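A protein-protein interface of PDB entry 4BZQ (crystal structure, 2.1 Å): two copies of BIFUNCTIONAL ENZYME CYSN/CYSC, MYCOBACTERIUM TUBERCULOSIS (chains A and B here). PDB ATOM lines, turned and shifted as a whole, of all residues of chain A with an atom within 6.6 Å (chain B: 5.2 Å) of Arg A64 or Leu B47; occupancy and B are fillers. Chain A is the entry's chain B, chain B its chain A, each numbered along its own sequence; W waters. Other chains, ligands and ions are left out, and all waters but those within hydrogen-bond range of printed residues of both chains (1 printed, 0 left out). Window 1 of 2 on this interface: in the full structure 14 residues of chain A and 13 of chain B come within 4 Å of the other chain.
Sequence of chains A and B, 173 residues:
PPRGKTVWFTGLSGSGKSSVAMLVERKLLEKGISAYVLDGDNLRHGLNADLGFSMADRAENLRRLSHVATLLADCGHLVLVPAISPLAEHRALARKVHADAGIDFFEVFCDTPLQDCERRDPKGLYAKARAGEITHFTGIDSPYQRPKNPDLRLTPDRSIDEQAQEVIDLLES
The backbone carbonyl oxygen (O) of Gly B46 is in hydrogen-bond range of the guanidinium group (NH1) of Arg A63 (3.2 Å).
NH1 of Arg A63 sits at hydrogen-bond distance from O of Leu B47 (3.1 Å).
The backbone NH (N) of Leu B47 sits at hydrogen-bond distance from a ring nitrogen (ND1) of His A67.
The side-chain carboxylate (OD1) of Asp B50 lies within salt-bridge range of the guanidinium group (NH2) of Arg A63, at 3.3 Å.
The guanidinium group (NH2) of Arg A64 lies within salt-bridge range of the side-chain carboxylate (OE2) of Glu B60.
The guanidinium group (NH1) of Arg B63 is in hydrogen-bond range of the backbone carbonyl oxygen (O) of Gly A46 (3.4 Å).
The backbone carbonyl oxygen (O) of Leu A47 is in hydrogen-bond range of the guanidinium group (NH2) of Arg B63.
The guanidinium group (NH2) of Arg B63 is in salt-bridge range of the side-chain carboxylate (OD1) of Asp A50 (3.3 Å).
The guanidinium group (NH2) of Arg B64 is in salt-bridge range of the side-chain carboxylate (OE2) of Glu A60, 3.8 Å away.
NH2 of Arg A64 lies close to NH2 of Arg B64 (3.3 Å).
The backbone carbonyl oxygen (O) of Leu B43 sits at hydrogen-bond distance from the backbone NH (N) of Asn B48 (2.9 Å).
The backbone carbonyl oxygen (O) of Leu B47 lies within hydrogen-bond range of the guanidinium group (NH1) of Arg B64 (3.2 Å).
The side-chain carboxylate (OE1) of Glu B60 lies within salt-bridge range of the guanidinium group (NE) of Arg B63.
NH1 of Arg A64 is in hydrogen-bond range of O of Leu A47.
NH1 of Arg A64 sits close to OD1 of Asn A48 (3.0 Å).
O of Arg A63 sits at hydrogen-bond distance from OG of Ser A66, at 2.7 Å.
Among the printed residues, merely in contact across the chains: His A67 with Gly B46 (3.4 Å), Arg A63 with Arg B64 (3.6 Å), Leu A47 with Arg B64 (3.8 Å), Arg A64 with Arg B63 (3.8 Å), Arg A64 with Leu B47 (3.9 Å) and Leu A71 with Leu B43 (3.9 Å).
Arg A64 touches just these residues of chain B: Leu B47 (3.9 Å), Glu B60 (3.9 Å), Arg B63 (3.8 Å) and Arg B64 (3.3 Å).
Leu B47 touches just these residues of chain A: Arg A63 (3.1 Å), Arg A64 (3.9 Å) and His A67 (3.5 Å).
Printed residues of chain B within 4 Å of His A67: Gly B46 and Leu B47.
Of the printed residues of chain A, Arg B63 touches Gly A46 (3.4 Å), Leu A47 (3.1 Å), Asp A50 (3.3 Å) and Arg A64 (3.8 Å).
Of the printed residues of chain B, Arg A63 touches Gly B46 (3.2 Å), Leu B47 (3.1 Å), Asp B50 (3.3 Å) and Arg B64 (3.6 Å).
Of the printed residues of chain A, Gly B46 touches Arg A63 and His A67.
Asn A48 touches none of the printed residues of chain B.
The nearest printed residue of chain B that does not touch Arg A64 is Asp B50 (5.4 Å).
Of the 11 printed residues of chain B, 7 touch a printed residue of chain A.
Printed residues of chain B that touch a printed residue of chain A: Leu B43, Gly B46, Leu B47, Asp B50, Glu B60, Arg B63 and Arg B64.
Along chain B the printed residues that touch a printed residue of chain A span positions 43 to 64.
Hydrophobic or aromatic side chains of chain A that line the printed part of chain B: Leu A47, His A67 and Leu A71.
Among the printed residues, 16 pairs touch across the chains.
Among the printed residues, Asp or Glu carboxylates within 4 Å of a Lys or Arg side-chain nitrogen of the other chain: Asp A50 with Arg B63 (3.3 Å), Glu A60 with Arg B64 (3.8 Å), Arg A63 with Asp B50 (3.3 Å) and Arg A64 with Glu B60 (3.9 Å).
Gly A46 touches Arg B63, and with the chains exchanged Arg A63 touches Gly B46.
Leu A47 touches Arg B63, and with the chains exchanged Arg A63 touches Leu B47.
Glu A60 touches Arg B64, and with the chains exchanged Arg A64 touches Glu B60.
Arg A63 touches Arg B64, and with the chains exchanged Arg A64 touches Arg B63.
Water W1 bridges NH1 of Arg B63 (2.5 Å) and O of Gly A46 (3.4 Å).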
ATOM      1  N   LEU A  38      19.325  -6.532  -9.548  1.00  0.00           N
ATOM      2  CA  LEU A  38      17.923  -6.346  -9.314  1.00  0.00           C
ATOM      3  C   LEU A  38      17.627  -6.929  -7.974  1.00  0.00           C
ATOM      4  O   LEU A  38      17.561  -8.145  -7.779  1.00  0.00           O
ATOM      5  CB  LEU A  38      17.149  -7.028 -10.398  1.00  0.00           C
ATOM      6  CG  LEU A  38      15.660  -6.841 -10.454  1.00  0.00           C
ATOM      7  CD1 LEU A  38      15.339  -5.467 -11.019  1.00  0.00           C
ATOM      8  CD2 LEU A  38      15.090  -7.901 -11.378  1.00  0.00           C
ATOM      9  N   GLY A  46       9.384   0.207  -4.614  1.00  0.00           N
ATOM     10  CA  GLY A  46       8.702   0.939  -5.701  1.00  0.00           C
ATOM     11  C   GLY A  46       7.692   0.033  -6.380  1.00  0.00           C
ATOM     12  O   GLY A  46       6.539  -0.074  -5.976  1.00  0.00           O
ATOM     13  N   LEU A  47       8.161  -0.697  -7.367  1.00  0.00           N
ATOM     14  CA  LEU A  47       7.324  -1.675  -8.000  1.00  0.00           C
ATOM     15  C   LEU A  47       6.606  -2.595  -7.009  1.00  0.00           C
ATOM     16  O   LEU A  47       5.467  -2.944  -7.234  1.00  0.00           O
ATOM     17  CB  LEU A  47       8.168  -2.544  -8.897  1.00  0.00           C
ATOM     18  CG  LEU A  47       7.453  -3.712  -9.562  1.00  0.00           C
ATOM     19  CD1 LEU A  47       6.430  -3.250 -10.592  1.00  0.00           C
ATOM     20  CD2 LEU A  47       8.442  -4.641 -10.198  1.00  0.00           C
ATOM     21  N   ASN A  48       7.310  -3.064  -5.979  1.00  0.00           N
ATOM     22  CA  ASN A  48       6.802  -4.072  -5.080  1.00  0.00           C
ATOM     23  C   ASN A  48       6.481  -3.518  -3.723  1.00  0.00           C
ATOM     24  O   ASN A  48       6.324  -4.283  -2.736  1.00  0.00           O
ATOM     25  CB  ASN A  48       7.787  -5.233  -4.946  1.00  0.00           C
ATOM     26  CG  ASN A  48       7.893  -6.045  -6.194  1.00  0.00           C
ATOM     27  OD1 ASN A  48       6.920  -6.203  -6.921  1.00  0.00           O
ATOM     28  ND2 ASN A  48       9.092  -6.538  -6.488  1.00  0.00           N
ATOM     29  N   ALA A  49       6.273  -2.210  -3.682  1.00  0.00           N
ATOM     30  CA  ALA A  49       5.913  -1.489  -2.475  1.00  0.00           C
ATOM     31  C   ALA A  49       4.570  -1.938  -1.860  1.00  0.00           C
ATOM     32  O   ALA A  49       4.251  -1.576  -0.743  1.00  0.00           O
ATOM     33  CB  ALA A  49       5.869   0.005  -2.766  1.00  0.00           C
ATOM     34  N   ASP A  50       3.783  -2.698  -2.600  1.00  0.00           N
ATOM     35  CA  ASP A  50       2.474  -3.165  -2.156  1.00  0.00           C
ATOM     36  C   ASP A  50       2.542  -4.591  -1.599  1.00  0.00           C
ATOM     37  O   ASP A  50       1.509  -5.200  -1.363  1.00  0.00           O
ATOM     38  CB  ASP A  50       1.525  -3.138  -3.371  1.00  0.00           C
ATOM     39  CG  ASP A  50       2.025  -4.041  -4.518  1.00  0.00           C
ATOM     40  OD1 ASP A  50       3.231  -3.974  -4.855  1.00  0.00           O
ATOM     41  OD2 ASP A  50       1.255  -4.867  -5.033  1.00  0.00           O
ATOM     42  N   LEU A  51       3.731  -5.156  -1.410  1.00  0.00           N
ATOM     43  CA  LEU A  51       3.833  -6.540  -0.941  1.00  0.00           C
ATOM     44  C   LEU A  51       4.545  -6.709   0.421  1.00  0.00           C
ATOM     45  O   LEU A  51       5.418  -5.915   0.758  1.00  0.00           O
ATOM     46  CB  LEU A  51       4.543  -7.384  -1.989  1.00  0.00           C
ATOM     47  CG  LEU A  51       3.905  -7.446  -3.376  1.00  0.00           C
ATOM     48  CD1 LEU A  51       4.862  -8.190  -4.291  1.00  0.00           C
ATOM     49  CD2 LEU A  51       2.524  -8.107  -3.354  1.00  0.00           C
ATOM     50  N   ALA A  59       6.081 -14.947  -2.862  1.00  0.00           N
ATOM     51  CA  ALA A  59       6.004 -15.603  -4.167  1.00  0.00           C
ATOM     52  C   ALA A  59       5.697 -14.558  -5.274  1.00  0.00           C
ATOM     53  O   ALA A  59       6.221 -14.666  -6.377  1.00  0.00           O
ATOM     54  CB  ALA A  59       4.960 -16.713  -4.200  1.00  0.00           C
ATOM     55  N   GLU A  60       4.843 -13.583  -4.957  1.00  0.00           N
ATOM     56  CA  GLU A  60       4.413 -12.524  -5.903  1.00  0.00           C
ATOM     57  C   GLU A  60       5.550 -11.564  -6.224  1.00  0.00           C
ATOM     58  O   GLU A  60       5.828 -11.279  -7.374  1.00  0.00           O
ATOM     59  CB  GLU A  60       3.183 -11.772  -5.341  1.00  0.00           C
ATOM     60  CG  GLU A  60       2.640 -10.594  -6.197  1.00  0.00           C
ATOM     61  CD  GLU A  60       2.416 -10.928  -7.629  1.00  0.00           C
ATOM     62  OE1 GLU A  60       2.237 -12.106  -8.013  1.00  0.00           O
ATOM     63  OE2 GLU A  60       2.397  -9.978  -8.441  1.00  0.00           O
ATOM     64  N   ASN A  61       6.215 -11.105  -5.172  1.00  0.00           N
ATOM     65  CA  ASN A  61       7.426 -10.326  -5.249  1.00  0.00           C
ATOM     66  C   ASN A  61       8.444 -10.994  -6.172  1.00  0.00           C
ATOM     67  O   ASN A  61       8.915 -10.401  -7.139  1.00  0.00           O
ATOM     68  CB  ASN A  61       8.016 -10.216  -3.863  1.00  0.00           C
ATOM     69  CG  ASN A  61       9.326  -9.476  -3.836  1.00  0.00           C
ATOM     70  OD1 ASN A  61       9.369  -8.279  -4.077  1.00  0.00           O
ATOM     71  ND2 ASN A  61      10.423 -10.184  -3.425  1.00  0.00           N
ATOM     72  N   LEU A  62       8.729 -12.250  -5.881  1.00  0.00           N
ATOM     73  CA  LEU A  62       9.678 -13.008  -6.612  1.00  0.00           C
ATOM     74  C   LEU A  62       9.173 -13.295  -8.015  1.00  0.00           C
ATOM     75  O   LEU A  62       9.987 -13.365  -8.946  1.00  0.00           O
ATOM     76  CB  LEU A  62      10.026 -14.333  -5.860  1.00  0.00           C
ATOM     77  CG  LEU A  62      10.695 -14.096  -4.478  1.00  0.00           C
ATOM     78  CD1 LEU A  62      10.744 -15.387  -3.653  1.00  0.00           C
ATOM     79  CD2 LEU A  62      12.055 -13.419  -4.594  1.00  0.00           C
ATOM     80  N   ARG A  63       7.871 -13.543  -8.174  1.00  0.00           N
ATOM     81  CA  ARG A  63       7.311 -13.741  -9.532  1.00  0.00           C
ATOM     82  C   ARG A  63       7.582 -12.471 -10.356  1.00  0.00           C
ATOM     83  O   ARG A  63       8.044 -12.534 -11.485  1.00  0.00           O
ATOM     84  CB  ARG A  63       5.784 -14.004  -9.483  1.00  0.00           C
ATOM     85  CG  ARG A  63       5.117 -14.304 -10.827  1.00  0.00           C
ATOM     86  CD  ARG A  63       3.598 -14.362 -10.680  1.00  0.00           C
ATOM     87  NE  ARG A  63       3.028 -13.029 -10.471  1.00  0.00           N
ATOM     88  CZ  ARG A  63       2.779 -12.144 -11.436  1.00  0.00           C
ATOM     89  NH1 ARG A  63       3.035 -12.418 -12.702  1.00  0.00           N
ATOM     90  NH2 ARG A  63       2.284 -10.961 -11.124  1.00  0.00           N
ATOM     91  N   ARG A  64       7.288 -11.326  -9.765  1.00  0.00           N
ATOM     92  CA  ARG A  64       7.486 -10.062 -10.448  1.00  0.00           C
ATOM     93  C   ARG A  64       8.956  -9.849 -10.767  1.00  0.00           C
ATOM     94  O   ARG A  64       9.298  -9.484 -11.889  1.00  0.00           O
ATOM     95  CB  ARG A  64       6.989  -8.919  -9.610  1.00  0.00           C
ATOM     96  CG  ARG A  64       5.489  -8.852  -9.509  1.00  0.00           C
ATOM     97  CD  ARG A  64       5.129  -7.595  -8.743  1.00  0.00           C
ATOM     98  NE  ARG A  64       3.767  -7.641  -8.270  1.00  0.00           N
ATOM     99  CZ  ARG A  64       3.231  -6.798  -7.396  1.00  0.00           C
ATOM    100  NH1 ARG A  64       3.927  -5.784  -6.912  1.00  0.00           N
ATOM    101  NH2 ARG A  64       1.972  -6.975  -7.029  1.00  0.00           N
ATOM    102  N   LEU A  65       9.809 -10.104  -9.773  1.00  0.00           N
ATOM    103  CA  LEU A  65      11.235  -9.961  -9.974  1.00  0.00           C
ATOM    104  C   LEU A  65      11.677 -10.807 -11.122  1.00  0.00           C
ATOM    105  O   LEU A  65      12.481 -10.360 -11.911  1.00  0.00           O
ATOM    106  CB  LEU A  65      12.064 -10.381  -8.763  1.00  0.00           C
ATOM    107  CG  LEU A  65      12.314  -9.346  -7.710  1.00  0.00           C
ATOM    108  CD1 LEU A  65      13.184  -9.968  -6.616  1.00  0.00           C
ATOM    109  CD2 LEU A  65      13.020  -8.173  -8.344  1.00  0.00           C
ATOM    110  N   SER A  66      11.179 -12.038 -11.195  1.00  0.00           N
ATOM    111  CA  SER A  66      11.614 -12.949 -12.216  1.00  0.00           C
ATOM    112  C   SER A  66      11.262 -12.378 -13.590  1.00  0.00           C
ATOM    113  O   SER A  66      12.084 -12.411 -14.498  1.00  0.00           O
ATOM    114  CB  SER A  66      11.052 -14.357 -11.975  1.00  0.00           C
ATOM    115  OG  SER A  66       9.704 -14.454 -12.375  1.00  0.00           O
ATOM    116  N   HIS A  67      10.077 -11.775 -13.741  1.00  0.00           N
ATOM    117  CA  HIS A  67       9.736 -11.154 -15.021  1.00  0.00           C
ATOM    118  C   HIS A  67      10.626  -9.980 -15.380  1.00  0.00           C
ATOM    119  O   HIS A  67      10.990  -9.800 -16.568  1.00  0.00           O
ATOM    120  CB  HIS A  67       8.257 -10.723 -15.047  1.00  0.00           C
ATOM    121  CG  HIS A  67       7.332 -11.881 -15.203  1.00  0.00           C
ATOM    122  ND1 HIS A  67       7.271 -12.609 -16.372  1.00  0.00           N
ATOM    123  CD2 HIS A  67       6.519 -12.510 -14.323  1.00  0.00           C
ATOM    124  CE1 HIS A  67       6.426 -13.611 -16.219  1.00  0.00           C
ATOM    125  NE2 HIS A  67       5.972 -13.586 -14.980  1.00  0.00           N
ATOM    126  N   VAL A  68      10.927  -9.150 -14.387  1.00  0.00           N
ATOM    127  CA  VAL A  68      11.706  -7.972 -14.656  1.00  0.00           C
ATOM    128  C   VAL A  68      13.128  -8.388 -15.044  1.00  0.00           C
ATOM    129  O   VAL A  68      13.727  -7.868 -16.026  1.00  0.00           O
ATOM    130  CB  VAL A  68      11.716  -7.020 -13.455  1.00  0.00           C
ATOM    131  CG1 VAL A  68      12.644  -5.839 -13.679  1.00  0.00           C
ATOM    132  CG2 VAL A  68      10.330  -6.503 -13.227  1.00  0.00           C
ATOM    133  N   ALA A  69      13.662  -9.388 -14.334  1.00  0.00           N
ATOM    134  CA  ALA A  69      14.947  -9.964 -14.726  1.00  0.00           C
ATOM    135  C   ALA A  69      14.906 -10.377 -16.194  1.00  0.00           C
ATOM    136  O   ALA A  69      15.827 -10.068 -16.940  1.00  0.00           O
ATOM    137  CB  ALA A  69      15.317 -11.168 -13.808  1.00  0.00           C
ATOM    138  N   LEU A  71      13.168  -9.318 -18.556  1.00  0.00           N
ATOM    139  CA  LEU A  71      13.056  -8.121 -19.388  1.00  0.00           C
ATOM    140  C   LEU A  71      14.402  -7.393 -19.514  1.00  0.00           C
ATOM    141  O   LEU A  71      14.826  -6.995 -20.627  1.00  0.00           O
ATOM    142  CB  LEU A  71      11.957  -7.171 -18.849  1.00  0.00           C
ATOM    143  CG  LEU A  71      10.537  -7.666 -19.061  1.00  0.00           C
ATOM    144  CD1 LEU A  71       9.636  -6.822 -18.193  1.00  0.00           C
ATOM    145  CD2 LEU A  71      10.139  -7.579 -20.507  1.00  0.00           C
ATOM    146  N   LEU B  43       2.967  -7.994 -22.043  1.00  0.00           N
ATOM    147  CA  LEU B  43       3.300  -8.143 -20.660  1.00  0.00           C
ATOM    148  C   LEU B  43       2.116  -8.679 -19.892  1.00  0.00           C
ATOM    149  O   LEU B  43       2.311  -9.300 -18.851  1.00  0.00           O
ATOM    150  CB  LEU B  43       3.779  -6.787 -20.121  1.00  0.00           C
ATOM    151  CG  LEU B  43       5.198  -6.494 -20.713  1.00  0.00           C
ATOM    152  CD1 LEU B  43       5.772  -5.302 -20.006  1.00  0.00           C
ATOM    153  CD2 LEU B  43       6.205  -7.628 -20.554  1.00  0.00           C
ATOM    154  N   HIS B  45       0.673 -11.157 -20.638  1.00  0.00           N
ATOM    155  CA  HIS B  45       0.899 -12.601 -20.683  1.00  0.00           C
ATOM    156  C   HIS B  45       2.009 -13.072 -19.771  1.00  0.00           C
ATOM    157  O   HIS B  45       2.315 -14.243 -19.757  1.00  0.00           O
ATOM    158  CB  HIS B  45       1.262 -13.012 -22.099  1.00  0.00           C
ATOM    159  CG  HIS B  45       0.156 -12.809 -23.066  1.00  0.00           C
ATOM    160  ND1 HIS B  45       0.053 -11.684 -23.865  1.00  0.00           N
ATOM    161  CD2 HIS B  45      -0.939 -13.558 -23.331  1.00  0.00           C
ATOM    162  CE1 HIS B  45      -1.050 -11.754 -24.589  1.00  0.00           C
ATOM    163  NE2 HIS B  45      -1.671 -12.879 -24.280  1.00  0.00           N
ATOM    164  N   GLY B  46       2.652 -12.180 -19.017  1.00  0.00           N
ATOM    165  CA  GLY B  46       3.664 -12.618 -18.072  1.00  0.00           C
ATOM    166  C   GLY B  46       3.574 -11.823 -16.796  1.00  0.00           C
ATOM    167  O   GLY B  46       2.839 -12.185 -15.869  1.00  0.00           O
ATOM    168  N   LEU B  47       4.345 -10.746 -16.726  1.00  0.00           N
ATOM    169  CA  LEU B  47       4.373  -9.925 -15.524  1.00  0.00           C
ATOM    170  C   LEU B  47       2.973  -9.560 -15.055  1.00  0.00           C
ATOM    171  O   LEU B  47       2.691  -9.599 -13.843  1.00  0.00           O
ATOM    172  CB  LEU B  47       5.120  -8.633 -15.756  1.00  0.00           C
ATOM    173  CG  LEU B  47       5.094  -7.640 -14.576  1.00  0.00           C
ATOM    174  CD1 LEU B  47       5.843  -8.149 -13.360  1.00  0.00           C
ATOM    175  CD2 LEU B  47       5.671  -6.303 -14.988  1.00  0.00           C
ATOM    176  N   ASN B  48       2.089  -9.221 -16.008  1.00  0.00           N
ATOM    177  CA  ASN B  48       0.795  -8.762 -15.618  1.00  0.00           C
ATOM    178  C   ASN B  48      -0.306  -9.760 -15.905  1.00  0.00           C
ATOM    179  O   ASN B  48      -1.479  -9.370 -16.058  1.00  0.00           O
ATOM    180  CB  ASN B  48       0.543  -7.422 -16.293  1.00  0.00           C
ATOM    181  CG  ASN B  48       1.438  -6.342 -15.760  1.00  0.00           C
ATOM    182  OD1 ASN B  48       1.723  -6.267 -14.531  1.00  0.00           O
ATOM    183  ND2 ASN B  48       1.940  -5.510 -16.665  1.00  0.00           N
ATOM    184  N   ALA B  49       0.069 -11.043 -15.985  1.00  0.00           N
ATOM    185  CA  ALA B  49      -0.857 -12.117 -16.307  1.00  0.00           C
ATOM    186  C   ALA B  49      -1.964 -12.266 -15.289  1.00  0.00           C
ATOM    187  O   ALA B  49      -2.978 -12.919 -15.567  1.00  0.00           O
ATOM    188  CB  ALA B  49      -0.117 -13.443 -16.442  1.00  0.00           C
ATOM    189  N   ASP B  50      -1.760 -11.687 -14.111  1.00  0.00           N
ATOM    190  CA  ASP B  50      -2.707 -11.791 -13.013  1.00  0.00           C
ATOM    191  C   ASP B  50      -3.746 -10.641 -13.052  1.00  0.00           C
ATOM    192  O   ASP B  50      -4.563 -10.514 -12.160  1.00  0.00           O
ATOM    193  CB  ASP B  50      -1.971 -11.734 -11.688  1.00  0.00           C
ATOM    194  CG  ASP B  50      -1.139 -10.453 -11.529  1.00  0.00           C
ATOM    195  OD1 ASP B  50      -0.502  -9.993 -12.511  1.00  0.00           O
ATOM    196  OD2 ASP B  50      -1.099  -9.887 -10.413  1.00  0.00           O
ATOM    197  N   GLU B  60      -3.302  -0.895 -11.853  1.00  0.00           N
ATOM    198  CA  GLU B  60      -2.199  -1.675 -11.293  1.00  0.00           C
ATOM    199  C   GLU B  60      -1.236  -2.050 -12.412  1.00  0.00           C
ATOM    200  O   GLU B  60      -0.036  -1.953 -12.236  1.00  0.00           O
ATOM    201  CB  GLU B  60      -2.778  -2.920 -10.584  1.00  0.00           C
ATOM    202  CG  GLU B  60      -1.768  -3.904 -10.015  1.00  0.00           C
ATOM    203  CD  GLU B  60      -0.709  -3.285  -9.118  1.00  0.00           C
ATOM    204  OE1 GLU B  60      -0.892  -2.182  -8.590  1.00  0.00           O
ATOM    205  OE2 GLU B  60       0.346  -3.929  -8.899  1.00  0.00           O
ATOM    206  N   ARG B  63       0.535   1.024 -13.305  1.00  0.00           N
ATOM    207  CA  ARG B  63       1.504   1.360 -12.212  1.00  0.00           C
ATOM    208  C   ARG B  63       2.785   0.511 -12.325  1.00  0.00           C
ATOM    209  O   ARG B  63       3.914   1.013 -12.288  1.00  0.00           O
ATOM    210  CB  ARG B  63       0.861   1.134 -10.844  1.00  0.00           C
ATOM    211  CG  ARG B  63       1.698   1.569  -9.619  1.00  0.00           C
ATOM    212  CD  ARG B  63       1.112   1.069  -8.312  1.00  0.00           C
ATOM    213  NE  ARG B  63       1.293  -0.378  -8.166  1.00  0.00           N
ATOM    214  CZ  ARG B  63       2.398  -1.002  -7.723  1.00  0.00           C
ATOM    215  NH1 ARG B  63       3.472  -0.321  -7.378  1.00  0.00           N
ATOM    216  NH2 ARG B  63       2.430  -2.329  -7.653  1.00  0.00           N
ATOM    217  N   ARG B  64       2.596  -0.778 -12.505  1.00  0.00           N
ATOM    218  CA  ARG B  64       3.685  -1.657 -12.660  1.00  0.00           C
ATOM    219  C   ARG B  64       4.513  -1.275 -13.839  1.00  0.00           C
ATOM    220  O   ARG B  64       5.744  -1.123 -13.730  1.00  0.00           O
ATOM    221  CB  ARG B  64       3.183  -3.067 -12.865  1.00  0.00           C
ATOM    222  CG  ARG B  64       2.629  -3.659 -11.611  1.00  0.00           C
ATOM    223  CD  ARG B  64       2.310  -5.128 -11.857  1.00  0.00           C
ATOM    224  NE  ARG B  64       1.459  -5.641 -10.807  1.00  0.00           N
ATOM    225  CZ  ARG B  64       0.862  -6.827 -10.843  1.00  0.00           C
ATOM    226  NH1 ARG B  64       1.000  -7.644 -11.899  1.00  0.00           N
ATOM    227  NH2 ARG B  64       0.126  -7.196  -9.801  1.00  0.00           N
ATOM    228  N   VAL B  68       8.631  -0.286 -14.237  1.00  0.00           N
ATOM    229  CA  VAL B  68       9.544  -1.049 -15.063  1.00  0.00           C
ATOM    230  C   VAL B  68      10.193  -0.124 -16.101  1.00  0.00           C
ATOM    231  O   VAL B  68      11.421  -0.143 -16.333  1.00  0.00           O
ATOM    232  CB  VAL B  68       8.829  -2.242 -15.716  1.00  0.00           C
ATOM    233  CG1 VAL B  68       9.736  -2.999 -16.648  1.00  0.00           C
ATOM    234  CG2 VAL B  68       8.314  -3.182 -14.663  1.00  0.00           C
HETATM  235  O   HOH W   1       4.082   2.055  -6.964  1.00  0.00           O
